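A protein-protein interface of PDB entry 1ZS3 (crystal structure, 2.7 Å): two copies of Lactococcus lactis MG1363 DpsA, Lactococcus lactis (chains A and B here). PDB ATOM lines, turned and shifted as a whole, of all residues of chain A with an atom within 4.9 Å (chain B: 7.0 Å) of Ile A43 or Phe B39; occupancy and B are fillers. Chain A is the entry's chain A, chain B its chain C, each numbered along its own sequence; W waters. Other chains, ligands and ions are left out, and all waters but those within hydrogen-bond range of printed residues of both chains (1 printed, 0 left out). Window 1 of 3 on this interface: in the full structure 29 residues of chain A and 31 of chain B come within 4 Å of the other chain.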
ATOM      1  N   PHE A  39     -19.873  10.074 -28.277  1.00  0.00           N
ATOM      2  CA  PHE A  39     -21.169   9.587 -27.850  1.00  0.00           C
ATOM      3  C   PHE A  39     -22.292  10.480 -28.267  1.00  0.00           C
ATOM      4  O   PHE A  39     -23.396   9.982 -28.526  1.00  0.00           O
ATOM      5  CB  PHE A  39     -21.214   9.338 -26.358  1.00  0.00           C
ATOM      6  CG  PHE A  39     -21.922   8.092 -26.021  1.00  0.00           C
ATOM      7  CD1 PHE A  39     -21.233   6.940 -25.717  1.00  0.00           C
ATOM      8  CD2 PHE A  39     -23.282   8.045 -26.095  1.00  0.00           C
ATOM      9  CE1 PHE A  39     -21.899   5.788 -25.429  1.00  0.00           C
ATOM     10  CE2 PHE A  39     -23.965   6.880 -25.821  1.00  0.00           C
ATOM     11  CZ  PHE A  39     -23.269   5.753 -25.481  1.00  0.00           C
ATOM     12  N   ILE A  40     -22.057  11.787 -28.376  1.00  0.00           N
ATOM     13  CA  ILE A  40     -23.158  12.663 -28.731  1.00  0.00           C
ATOM     14  C   ILE A  40     -23.366  12.548 -30.220  1.00  0.00           C
ATOM     15  O   ILE A  40     -24.501  12.529 -30.648  1.00  0.00           O
ATOM     16  CB  ILE A  40     -22.928  14.146 -28.189  1.00  0.00           C
ATOM     17  CG1 ILE A  40     -23.851  14.408 -27.011  1.00  0.00           C
ATOM     18  CG2 ILE A  40     -23.205  15.187 -29.229  1.00  0.00           C
ATOM     19  CD1 ILE A  40     -23.633  13.472 -25.869  1.00  0.00           C
ATOM     20  N   GLU A  41     -22.293  12.469 -31.003  1.00  0.00           N
ATOM     21  CA  GLU A  41     -22.402  12.098 -32.416  1.00  0.00           C
ATOM     22  C   GLU A  41     -23.162  10.790 -32.581  1.00  0.00           C
ATOM     23  O   GLU A  41     -24.030  10.725 -33.397  1.00  0.00           O
ATOM     24  CB  GLU A  41     -21.037  11.943 -33.051  1.00  0.00           C
ATOM     25  CG  GLU A  41     -21.096  12.200 -34.529  1.00  0.00           C
ATOM     26  CD  GLU A  41     -21.081  13.661 -34.882  1.00  0.00           C
ATOM     27  OE1 GLU A  41     -22.114  14.152 -35.384  1.00  0.00           O
ATOM     28  OE2 GLU A  41     -20.034  14.304 -34.650  1.00  0.00           O
ATOM     29  N   ASN A  42     -22.854   9.765 -31.812  1.00  0.00           N
ATOM     30  CA  ASN A  42     -23.603   8.525 -31.842  1.00  0.00           C
ATOM     31  C   ASN A  42     -25.111   8.734 -31.850  1.00  0.00           C
ATOM     32  O   ASN A  42     -25.847   8.101 -32.617  1.00  0.00           O
ATOM     33  CB  ASN A  42     -23.185   7.617 -30.671  1.00  0.00           C
ATOM     34  CG  ASN A  42     -23.968   6.336 -30.615  1.00  0.00           C
ATOM     35  OD1 ASN A  42     -24.446   5.943 -29.565  1.00  0.00           O
ATOM     36  ND2 ASN A  42     -24.080   5.674 -31.747  1.00  0.00           N
ATOM     37  N   ILE A  43     -25.572   9.614 -30.983  1.00  0.00           N
ATOM     38  CA  ILE A  43     -27.006   9.877 -30.828  1.00  0.00           C
ATOM     39  C   ILE A  43     -27.505  10.642 -32.045  1.00  0.00           C
ATOM     40  O   ILE A  43     -28.571  10.385 -32.585  1.00  0.00           O
ATOM     41  CB  ILE A  43     -27.289  10.668 -29.524  1.00  0.00           C
ATOM     42  CG1 ILE A  43     -26.499  10.052 -28.356  1.00  0.00           C
ATOM     43  CG2 ILE A  43     -28.793  10.771 -29.290  1.00  0.00           C
ATOM     44  CD1 ILE A  43     -27.326   9.555 -27.196  1.00  0.00           C
ATOM     45  N   ARG A  44     -26.704  11.570 -32.498  1.00  0.00           N
ATOM     46  CA  ARG A  44     -27.033  12.374 -33.654  1.00  0.00           C
ATOM     47  C   ARG A  44     -27.140  11.538 -34.904  1.00  0.00           C
ATOM     48  O   ARG A  44     -27.979  11.816 -35.756  1.00  0.00           O
ATOM     49  CB  ARG A  44     -25.965  13.473 -33.829  1.00  0.00           C
ATOM     50  CG  ARG A  44     -26.270  14.802 -33.122  1.00  0.00           C
ATOM     51  CD  ARG A  44     -26.900  15.822 -34.046  1.00  0.00           C
ATOM     52  NE  ARG A  44     -25.903  16.340 -34.993  1.00  0.00           N
ATOM     53  CZ  ARG A  44     -26.143  16.656 -36.268  1.00  0.00           C
ATOM     54  NH1 ARG A  44     -27.351  16.527 -36.828  1.00  0.00           N
ATOM     55  NH2 ARG A  44     -25.126  17.105 -36.984  1.00  0.00           N
ATOM     56  N   LEU A  45     -26.290  10.512 -35.008  1.00  0.00           N
ATOM     57  CA  LEU A  45     -26.205   9.612 -36.152  1.00  0.00           C
ATOM     58  C   LEU A  45     -27.228   8.560 -35.988  1.00  0.00           C
ATOM     59  O   LEU A  45     -27.757   8.088 -36.972  1.00  0.00           O
ATOM     60  CB  LEU A  45     -24.823   8.946 -36.243  1.00  0.00           C
ATOM     61  CG  LEU A  45     -23.704   9.882 -36.735  1.00  0.00           C
ATOM     62  CD1 LEU A  45     -22.349   9.390 -36.355  1.00  0.00           C
ATOM     63  CD2 LEU A  45     -23.793  10.100 -38.263  1.00  0.00           C
ATOM     64  N   THR A  46     -27.513   8.147 -34.747  1.00  0.00           N
ATOM     65  CA  THR A  46     -28.680   7.351 -34.454  1.00  0.00           C
ATOM     66  C   THR A  46     -29.981   8.044 -34.861  1.00  0.00           C
ATOM     67  O   THR A  46     -30.876   7.411 -35.441  1.00  0.00           O
ATOM     68  CB  THR A  46     -28.742   7.046 -32.979  1.00  0.00           C
ATOM     69  OG1 THR A  46     -27.631   6.219 -32.607  1.00  0.00           O
ATOM     70  CG2 THR A  46     -29.946   6.199 -32.650  1.00  0.00           C
ATOM     71  N   GLN A  47     -30.124   9.337 -34.562  1.00  0.00           N
ATOM     72  CA  GLN A  47     -31.309  10.080 -35.005  1.00  0.00           C
ATOM     73  C   GLN A  47     -31.402  10.102 -36.531  1.00  0.00           C
ATOM     74  O   GLN A  47     -32.450   9.766 -37.086  1.00  0.00           O
ATOM     75  CB  GLN A  47     -31.266  11.519 -34.466  1.00  0.00           C
ATOM     76  CG  GLN A  47     -32.258  12.494 -35.166  1.00  0.00           C
ATOM     77  CD  GLN A  47     -32.254  13.880 -34.561  1.00  0.00           C
ATOM     78  OE1 GLN A  47     -31.384  14.695 -34.889  1.00  0.00           O
ATOM     79  NE2 GLN A  47     -33.217  14.149 -33.682  1.00  0.00           N
ATOM     80  N   GLU A 102     -27.105  18.928 -30.739  1.00  0.00           N
ATOM     81  CA  GLU A 102     -28.308  18.172 -31.082  1.00  0.00           C
ATOM     82  C   GLU A 102     -29.413  19.123 -31.538  1.00  0.00           C
ATOM     83  O   GLU A 102     -29.173  20.301 -31.655  1.00  0.00           O
ATOM     84  CB  GLU A 102     -28.729  17.288 -29.942  1.00  0.00           C
ATOM     85  CG  GLU A 102     -27.649  16.295 -29.606  1.00  0.00           C
ATOM     86  CD  GLU A 102     -28.033  15.471 -28.428  1.00  0.00           C
ATOM     87  OE1 GLU A 102     -28.993  14.662 -28.565  1.00  0.00           O
ATOM     88  OE2 GLU A 102     -27.359  15.640 -27.377  1.00  0.00           O
ATOM     89  N   VAL B  34     -40.301   3.492 -23.290  1.00  0.00           N
ATOM     90  CA  VAL B  34     -39.490   2.280 -23.404  1.00  0.00           C
ATOM     91  C   VAL B  34     -38.182   2.540 -24.164  1.00  0.00           C
ATOM     92  O   VAL B  34     -37.116   2.090 -23.747  1.00  0.00           O
ATOM     93  CB  VAL B  34     -40.267   1.176 -24.088  1.00  0.00           C
ATOM     94  CG1 VAL B  34     -39.539  -0.122 -24.012  1.00  0.00           C
ATOM     95  CG2 VAL B  34     -41.664   0.979 -23.467  1.00  0.00           C
ATOM     96  N   LEU B  35     -38.262   3.295 -25.259  1.00  0.00           N
ATOM     97  CA  LEU B  35     -37.092   3.633 -26.025  1.00  0.00           C
ATOM     98  C   LEU B  35     -36.151   4.535 -25.280  1.00  0.00           C
ATOM     99  O   LEU B  35     -34.916   4.373 -25.390  1.00  0.00           O
ATOM    100  CB  LEU B  35     -37.480   4.299 -27.354  1.00  0.00           C
ATOM    101  CG  LEU B  35     -38.325   3.414 -28.303  1.00  0.00           C
ATOM    102  CD1 LEU B  35     -38.588   4.239 -29.521  1.00  0.00           C
ATOM    103  CD2 LEU B  35     -37.606   2.106 -28.670  1.00  0.00           C
ATOM    104  N   SER B  36     -36.701   5.490 -24.535  1.00  0.00           N
ATOM    105  CA  SER B  36     -35.832   6.453 -23.828  1.00  0.00           C
ATOM    106  C   SER B  36     -35.093   5.769 -22.691  1.00  0.00           C
ATOM    107  O   SER B  36     -33.957   6.098 -22.425  1.00  0.00           O
ATOM    108  CB  SER B  36     -36.630   7.657 -23.350  1.00  0.00           C
ATOM    109  OG  SER B  36     -36.811   8.606 -24.392  1.00  0.00           O
ATOM    110  N   ASN B  37     -35.755   4.811 -22.048  1.00  0.00           N
ATOM    111  CA  ASN B  37     -35.137   3.902 -21.104  1.00  0.00           C
ATOM    112  C   ASN B  37     -34.033   2.995 -21.675  1.00  0.00           C
ATOM    113  O   ASN B  37     -33.037   2.680 -21.014  1.00  0.00           O
ATOM    114  CB  ASN B  37     -36.224   3.002 -20.454  1.00  0.00           C
ATOM    115  CG  ASN B  37     -37.113   3.730 -19.444  1.00  0.00           C
ATOM    116  OD1 ASN B  37     -36.798   4.845 -19.052  1.00  0.00           O
ATOM    117  ND2 ASN B  37     -38.195   3.070 -19.046  1.00  0.00           N
ATOM    118  N   LEU B  38     -34.252   2.531 -22.915  1.00  0.00           N
ATOM    119  CA  LEU B  38     -33.278   1.685 -23.600  1.00  0.00           C
ATOM    120  C   LEU B  38     -32.001   2.464 -23.829  1.00  0.00           C
ATOM    121  O   LEU B  38     -30.922   1.965 -23.569  1.00  0.00           O
ATOM    122  CB  LEU B  38     -33.788   1.155 -24.951  1.00  0.00           C
ATOM    123  CG  LEU B  38     -34.783   0.011 -24.928  1.00  0.00           C
ATOM    124  CD1 LEU B  38     -35.449  -0.145 -26.303  1.00  0.00           C
ATOM    125  CD2 LEU B  38     -34.147  -1.291 -24.403  1.00  0.00           C
ATOM    126  N   PHE B  39     -32.100   3.699 -24.333  1.00  0.00           N
ATOM    127  CA  PHE B  39     -30.886   4.442 -24.598  1.00  0.00           C
ATOM    128  C   PHE B  39     -30.102   4.784 -23.345  1.00  0.00           C
ATOM    129  O   PHE B  39     -28.883   4.629 -23.291  1.00  0.00           O
ATOM    130  CB  PHE B  39     -31.089   5.691 -25.453  1.00  0.00           C
ATOM    131  CG  PHE B  39     -29.971   5.887 -26.419  1.00  0.00           C
ATOM    132  CD1 PHE B  39     -30.139   5.626 -27.772  1.00  0.00           C
ATOM    133  CD2 PHE B  39     -28.703   6.220 -25.961  1.00  0.00           C
ATOM    134  CE1 PHE B  39     -29.070   5.767 -28.664  1.00  0.00           C
ATOM    135  CE2 PHE B  39     -27.630   6.357 -26.846  1.00  0.00           C
ATOM    136  CZ  PHE B  39     -27.815   6.137 -28.205  1.00  0.00           C
ATOM    137  N   ILE B  40     -30.797   5.267 -22.297  1.00  0.00           N
ATOM    138  CA  ILE B  40     -30.164   5.624 -21.036  1.00  0.00           C
ATOM    139  C   ILE B  40     -29.604   4.359 -20.393  1.00  0.00           C
ATOM    140  O   ILE B  40     -28.475   4.387 -19.900  1.00  0.00           O
ATOM    141  CB  ILE B  40     -31.112   6.478 -20.049  1.00  0.00           C
ATOM    142  CG1 ILE B  40     -31.012   7.985 -20.321  1.00  0.00           C
ATOM    143  CG2 ILE B  40     -30.687   6.373 -18.600  1.00  0.00           C
ATOM    144  CD1 ILE B  40     -30.732   8.332 -21.729  1.00  0.00           C
ATOM    145  N   GLU B  41     -30.323   3.239 -20.456  1.00  0.00           N
ATOM    146  CA  GLU B  41     -29.773   1.972 -19.930  1.00  0.00           C
ATOM    147  C   GLU B  41     -28.489   1.537 -20.676  1.00  0.00           C
ATOM    148  O   GLU B  41     -27.578   0.958 -20.082  1.00  0.00           O
ATOM    149  CB  GLU B  41     -30.798   0.838 -19.971  1.00  0.00           C
ATOM    150  CG  GLU B  41     -30.333  -0.362 -19.164  1.00  0.00           C
ATOM    151  CD  GLU B  41     -30.644  -0.169 -17.680  1.00  0.00           C
ATOM    152  OE1 GLU B  41     -29.829   0.438 -16.930  1.00  0.00           O
ATOM    153  OE2 GLU B  41     -31.739  -0.583 -17.272  1.00  0.00           O
ATOM    154  N   ASN B  42     -28.426   1.843 -21.975  1.00  0.00           N
ATOM    155  CA  ASN B  42     -27.253   1.561 -22.776  1.00  0.00           C
ATOM    156  C   ASN B  42     -26.052   2.354 -22.266  1.00  0.00           C
ATOM    157  O   ASN B  42     -24.884   1.911 -22.379  1.00  0.00           O
ATOM    158  CB  ASN B  42     -27.546   1.911 -24.225  1.00  0.00           C
ATOM    159  CG  ASN B  42     -26.323   2.003 -25.088  1.00  0.00           C
ATOM    160  OD1 ASN B  42     -25.952   3.085 -25.512  1.00  0.00           O
ATOM    161  ND2 ASN B  42     -25.665   0.883 -25.372  1.00  0.00           N
ATOM    162  N   ILE B  43     -26.328   3.531 -21.703  1.00  0.00           N
ATOM    163  CA  ILE B  43     -25.235   4.363 -21.216  1.00  0.00           C
ATOM    164  C   ILE B  43     -24.679   3.799 -19.908  1.00  0.00           C
ATOM    165  O   ILE B  43     -23.469   3.789 -19.660  1.00  0.00           O
ATOM    166  CB  ILE B  43     -25.668   5.789 -21.054  1.00  0.00           C
ATOM    167  CG1 ILE B  43     -26.321   6.284 -22.362  1.00  0.00           C
ATOM    168  CG2 ILE B  43     -24.506   6.589 -20.626  1.00  0.00           C
ATOM    169  CD1 ILE B  43     -25.759   7.568 -22.950  1.00  0.00           C
ATOM    170  N   ARG B  44     -25.582   3.292 -19.089  1.00  0.00           N
ATOM    171  CA  ARG B  44     -25.197   2.734 -17.828  1.00  0.00           C
ATOM    172  C   ARG B  44     -24.410   1.499 -18.060  1.00  0.00           C
ATOM    173  O   ARG B  44     -23.358   1.317 -17.441  1.00  0.00           O
ATOM    174  CB  ARG B  44     -26.430   2.412 -16.970  1.00  0.00           C
ATOM    175  CG  ARG B  44     -27.218   3.625 -16.449  1.00  0.00           C
ATOM    176  CD  ARG B  44     -27.226   3.761 -14.958  1.00  0.00           C
ATOM    177  NE  ARG B  44     -27.692   2.545 -14.282  1.00  0.00           N
ATOM    178  CZ  ARG B  44     -26.981   1.816 -13.416  1.00  0.00           C
ATOM    179  NH1 ARG B  44     -25.747   2.146 -13.097  1.00  0.00           N
ATOM    180  NH2 ARG B  44     -27.509   0.730 -12.855  1.00  0.00           N
ATOM    181  N   GLU B  68     -29.503  -3.537 -26.254  1.00  0.00           N
ATOM    182  CA  GLU B  68     -30.435  -2.439 -26.007  1.00  0.00           C
ATOM    183  C   GLU B  68     -30.469  -1.512 -27.222  1.00  0.00           C
ATOM    184  O   GLU B  68     -31.545  -1.081 -27.616  1.00  0.00           O
ATOM    185  CB  GLU B  68     -30.092  -1.684 -24.714  1.00  0.00           C
ATOM    186  CG  GLU B  68     -30.103  -2.582 -23.485  1.00  0.00           C
ATOM    187  CD  GLU B  68     -31.462  -2.758 -22.876  1.00  0.00           C
ATOM    188  OE1 GLU B  68     -31.864  -1.847 -22.144  1.00  0.00           O
ATOM    189  OE2 GLU B  68     -32.131  -3.788 -23.114  1.00  0.00           O
ATOM    190  N   VAL B  69     -29.311  -1.199 -27.791  1.00  0.00           N
ATOM    191  CA  VAL B  69     -29.254  -0.421 -29.027  1.00  0.00           C
ATOM    192  C   VAL B  69     -29.862  -1.145 -30.223  1.00  0.00           C
ATOM    193  O   VAL B  69     -30.451  -0.526 -31.080  1.00  0.00           O
ATOM    194  CB  VAL B  69     -27.842   0.040 -29.334  1.00  0.00           C
ATOM    195  CG1 VAL B  69     -27.800   0.924 -30.561  1.00  0.00           C
ATOM    196  CG2 VAL B  69     -27.318   0.794 -28.150  1.00  0.00           C
ATOM    197  N   PHE B  72     -33.471  -0.748 -29.655  1.00  0.00           N
ATOM    198  CA  PHE B  72     -33.836   0.637 -29.895  1.00  0.00           C
ATOM    199  C   PHE B  72     -34.171   0.733 -31.360  1.00  0.00           C
ATOM    200  O   PHE B  72     -35.223   1.238 -31.740  1.00  0.00           O
ATOM    201  CB  PHE B  72     -32.683   1.580 -29.541  1.00  0.00           C
ATOM    202  CG  PHE B  72     -33.035   3.051 -29.681  1.00  0.00           C
ATOM    203  CD1 PHE B  72     -32.813   3.732 -30.876  1.00  0.00           C
ATOM    204  CD2 PHE B  72     -33.596   3.752 -28.627  1.00  0.00           C
ATOM    205  CE1 PHE B  72     -33.127   5.109 -31.016  1.00  0.00           C
ATOM    206  CE2 PHE B  72     -33.923   5.127 -28.761  1.00  0.00           C
ATOM    207  CZ  PHE B  72     -33.673   5.808 -29.956  1.00  0.00           C
ATOM    208  N   PHE B  73     -33.291   0.193 -32.186  1.00  0.00           N
ATOM    209  CA  PHE B  73     -33.373   0.382 -33.632  1.00  0.00           C
ATOM    210  C   PHE B  73     -34.511  -0.414 -34.214  1.00  0.00           C
ATOM    211  O   PHE B  73     -35.261   0.098 -35.045  1.00  0.00           O
ATOM    212  CB  PHE B  73     -32.044   0.017 -34.286  1.00  0.00           C
ATOM    213  CG  PHE B  73     -31.102   1.190 -34.437  1.00  0.00           C
ATOM    214  CD1 PHE B  73     -29.834   1.139 -33.890  1.00  0.00           C
ATOM    215  CD2 PHE B  73     -31.466   2.312 -35.155  1.00  0.00           C
ATOM    216  CE1 PHE B  73     -28.962   2.163 -34.026  1.00  0.00           C
ATOM    217  CE2 PHE B  73     -30.606   3.366 -35.282  1.00  0.00           C
ATOM    218  CZ  PHE B  73     -29.344   3.295 -34.723  1.00  0.00           C
ATOM    219  N   PRO B  87     -38.465   9.305 -30.023  1.00  0.00           N
ATOM    220  CA  PRO B  87     -37.492  10.230 -29.397  1.00  0.00           C
ATOM    221  C   PRO B  87     -36.089   9.992 -29.896  1.00  0.00           C
ATOM    222  O   PRO B  87     -35.606   8.865 -29.899  1.00  0.00           O
ATOM    223  CB  PRO B  87     -37.605   9.924 -27.901  1.00  0.00           C
ATOM    224  CG  PRO B  87     -38.220   8.551 -27.825  1.00  0.00           C
ATOM    225  CD  PRO B  87     -39.039   8.356 -29.053  1.00  0.00           C
ATOM    226  N   SER B  88     -35.452  11.074 -30.335  1.00  0.00           N
ATOM    227  CA  SER B  88     -34.193  11.002 -31.099  1.00  0.00           C
ATOM    228  C   SER B  88     -33.073  11.888 -30.511  1.00  0.00           C
ATOM    229  O   SER B  88     -32.100  12.136 -31.213  1.00  0.00           O
ATOM    230  CB  SER B  88     -34.472  11.453 -32.535  1.00  0.00           C
ATOM    231  OG  SER B  88     -35.185  12.679 -32.558  1.00  0.00           O
ATOM    232  N   THR B  89     -33.179  12.395 -29.280  1.00  0.00           N
ATOM    233  CA  THR B  89     -32.075  13.225 -28.695  1.00  0.00           C
ATOM    234  C   THR B  89     -31.880  13.020 -27.197  1.00  0.00           C
ATOM    235  O   THR B  89     -32.729  12.439 -26.534  1.00  0.00           O
ATOM    236  CB  THR B  89     -32.383  14.730 -28.889  1.00  0.00           C
ATOM    237  OG1 THR B  89     -33.660  15.025 -28.332  1.00  0.00           O
ATOM    238  CG2 THR B  89     -32.505  15.114 -30.338  1.00  0.00           C
ATOM    239  N   THR B  90     -30.773  13.537 -26.670  1.00  0.00           N
ATOM    240  CA  THR B  90     -30.475  13.504 -25.224  1.00  0.00           C
ATOM    241  C   THR B  90     -31.547  14.202 -24.382  1.00  0.00           C
ATOM    242  O   THR B  90     -32.017  13.651 -23.386  1.00  0.00           O
ATOM    243  CB  THR B  90     -29.058  14.107 -24.904  1.00  0.00           C
ATOM    244  OG1 THR B  90     -28.209  14.032 -26.049  1.00  0.00           O
ATOM    245  CG2 THR B  90     -28.334  13.239 -23.938  1.00  0.00           C
ATOM    246  N   PHE B  93     -34.651  11.993 -24.493  1.00  0.00           N
ATOM    247  CA  PHE B  93     -34.426  10.788 -23.690  1.00  0.00           C
ATOM    248  C   PHE B  93     -34.562  11.108 -22.204  1.00  0.00           C
ATOM    249  O   PHE B  93     -35.077  10.298 -21.416  1.00  0.00           O
ATOM    250  CB  PHE B  93     -33.022  10.162 -23.962  1.00  0.00           C
ATOM    251  CG  PHE B  93     -32.814   9.634 -25.373  1.00  0.00           C
ATOM    252  CD1 PHE B  93     -33.866   9.128 -26.141  1.00  0.00           C
ATOM    253  CD2 PHE B  93     -31.541   9.676 -25.945  1.00  0.00           C
ATOM    254  CE1 PHE B  93     -33.648   8.669 -27.419  1.00  0.00           C
ATOM    255  CE2 PHE B  93     -31.303   9.204 -27.245  1.00  0.00           C
ATOM    256  CZ  PHE B  93     -32.370   8.703 -27.983  1.00  0.00           C
HETATM  257  O   HOH W   1     -29.544  14.104 -31.929  1.00  0.00           O
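Of the printed residues of chain B, Ile A43 touches Phe B39 (3.2 Å) and Phe B93 (3.6 Å). Phe B39 touches three residues of chain A. Of the printed residues of chain B, Gln A47 touches Ser B88 (2.7 Å) and Thr B89 (3.6 Å). Printed residues of chain B within 4 Å of Thr A46: Phe B72 and Phe B73. Of the printed residues of chain B, Asn A42 touches Phe B39. Of the printed residues of chain B, Glu A102 touches Thr B89 and Thr B90. Printed residues of chain B within 4 Å of Phe A39: Phe B39, Asn B42 and Ile B43. Asn B37 touches none of the printed residues of chain A. The nearest residue of chain B that does not touch Ile A43 is Ser B88 (4.1 Å). The nearest residue of chain A that does not touch Phe B39 is Thr A46 (4.1 Å).
CE2 of Phe B39 touches CE2 of Phe A39 (3.8 Å). Phe A39 touches Asn B42 (CZ to OD1, 3.8 Å). CD1 of Ile B43 touches CE2 of Phe A39 (3.5 Å). CZ of Phe B39 touches OD1 of Asn A42, 3.6 Å away. Ile A43 touches Phe B39 (CD1 to CE2, 3.2 Å). Phe B93 touches Ile A43. Phe B72 touches Thr A46. Thr A46 touches Phe B73 (CG2 to CZ, 3.6 Å). Thr B89 touches Gln A47. Glu A102 touches Thr B89.
Water W1 bridges the backbone carbonyl oxygen of Ser B88 and the side-chain carboxylate of Glu A102.
Phe B39 touches its own counterpart, Phe A39. Phe A39 touches Asn B42, and with the chains exchanged Asn A42 touches Phe B39. Phe A39 touches Ile B43, and with the chains exchanged Ile A43 touches Phe B39. Positions printed for both chains: 39, 40, 41, 42, 43 and 44. Of the 12 pairs that touch across the chains among the printed residues, 5 have their exchanged pair printed and touching as well.
NE2 of Gln A47 is in hydrogen-bond range of OG of Ser B88, at 2.7 Å. The side-chain carboxylate (OE1) of Glu A102 is in hydrogen-bond range of the side-chain hydroxyl (OG1) of Thr B90 (2.7 Å).
The backbone carbonyl oxygen (O) of Asn A42 is in hydrogen-bond range of the side-chain hydroxyl (OG1) of Thr A46.
Of the 20 printed residues of chain B, 9 touch a printed residue of chain A. Hydrophobic or aromatic side chains of chain B within 4 Å of the printed part of chain A: Phe B39, Ile B43, Phe B72, Phe B73 and Phe B93. Of the 10 printed residues of chain A, 6 touch a printed residue of chain B. Along chain A the printed residues that touch a printed residue of chain B span positions 39 to 102. Among the printed residues, 12 pairs touch across the chains. Among the printed residues, no Asp or Glu carboxylate lies within 4 Å of a Lys or Arg side-chain nitrogen of the other chain.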
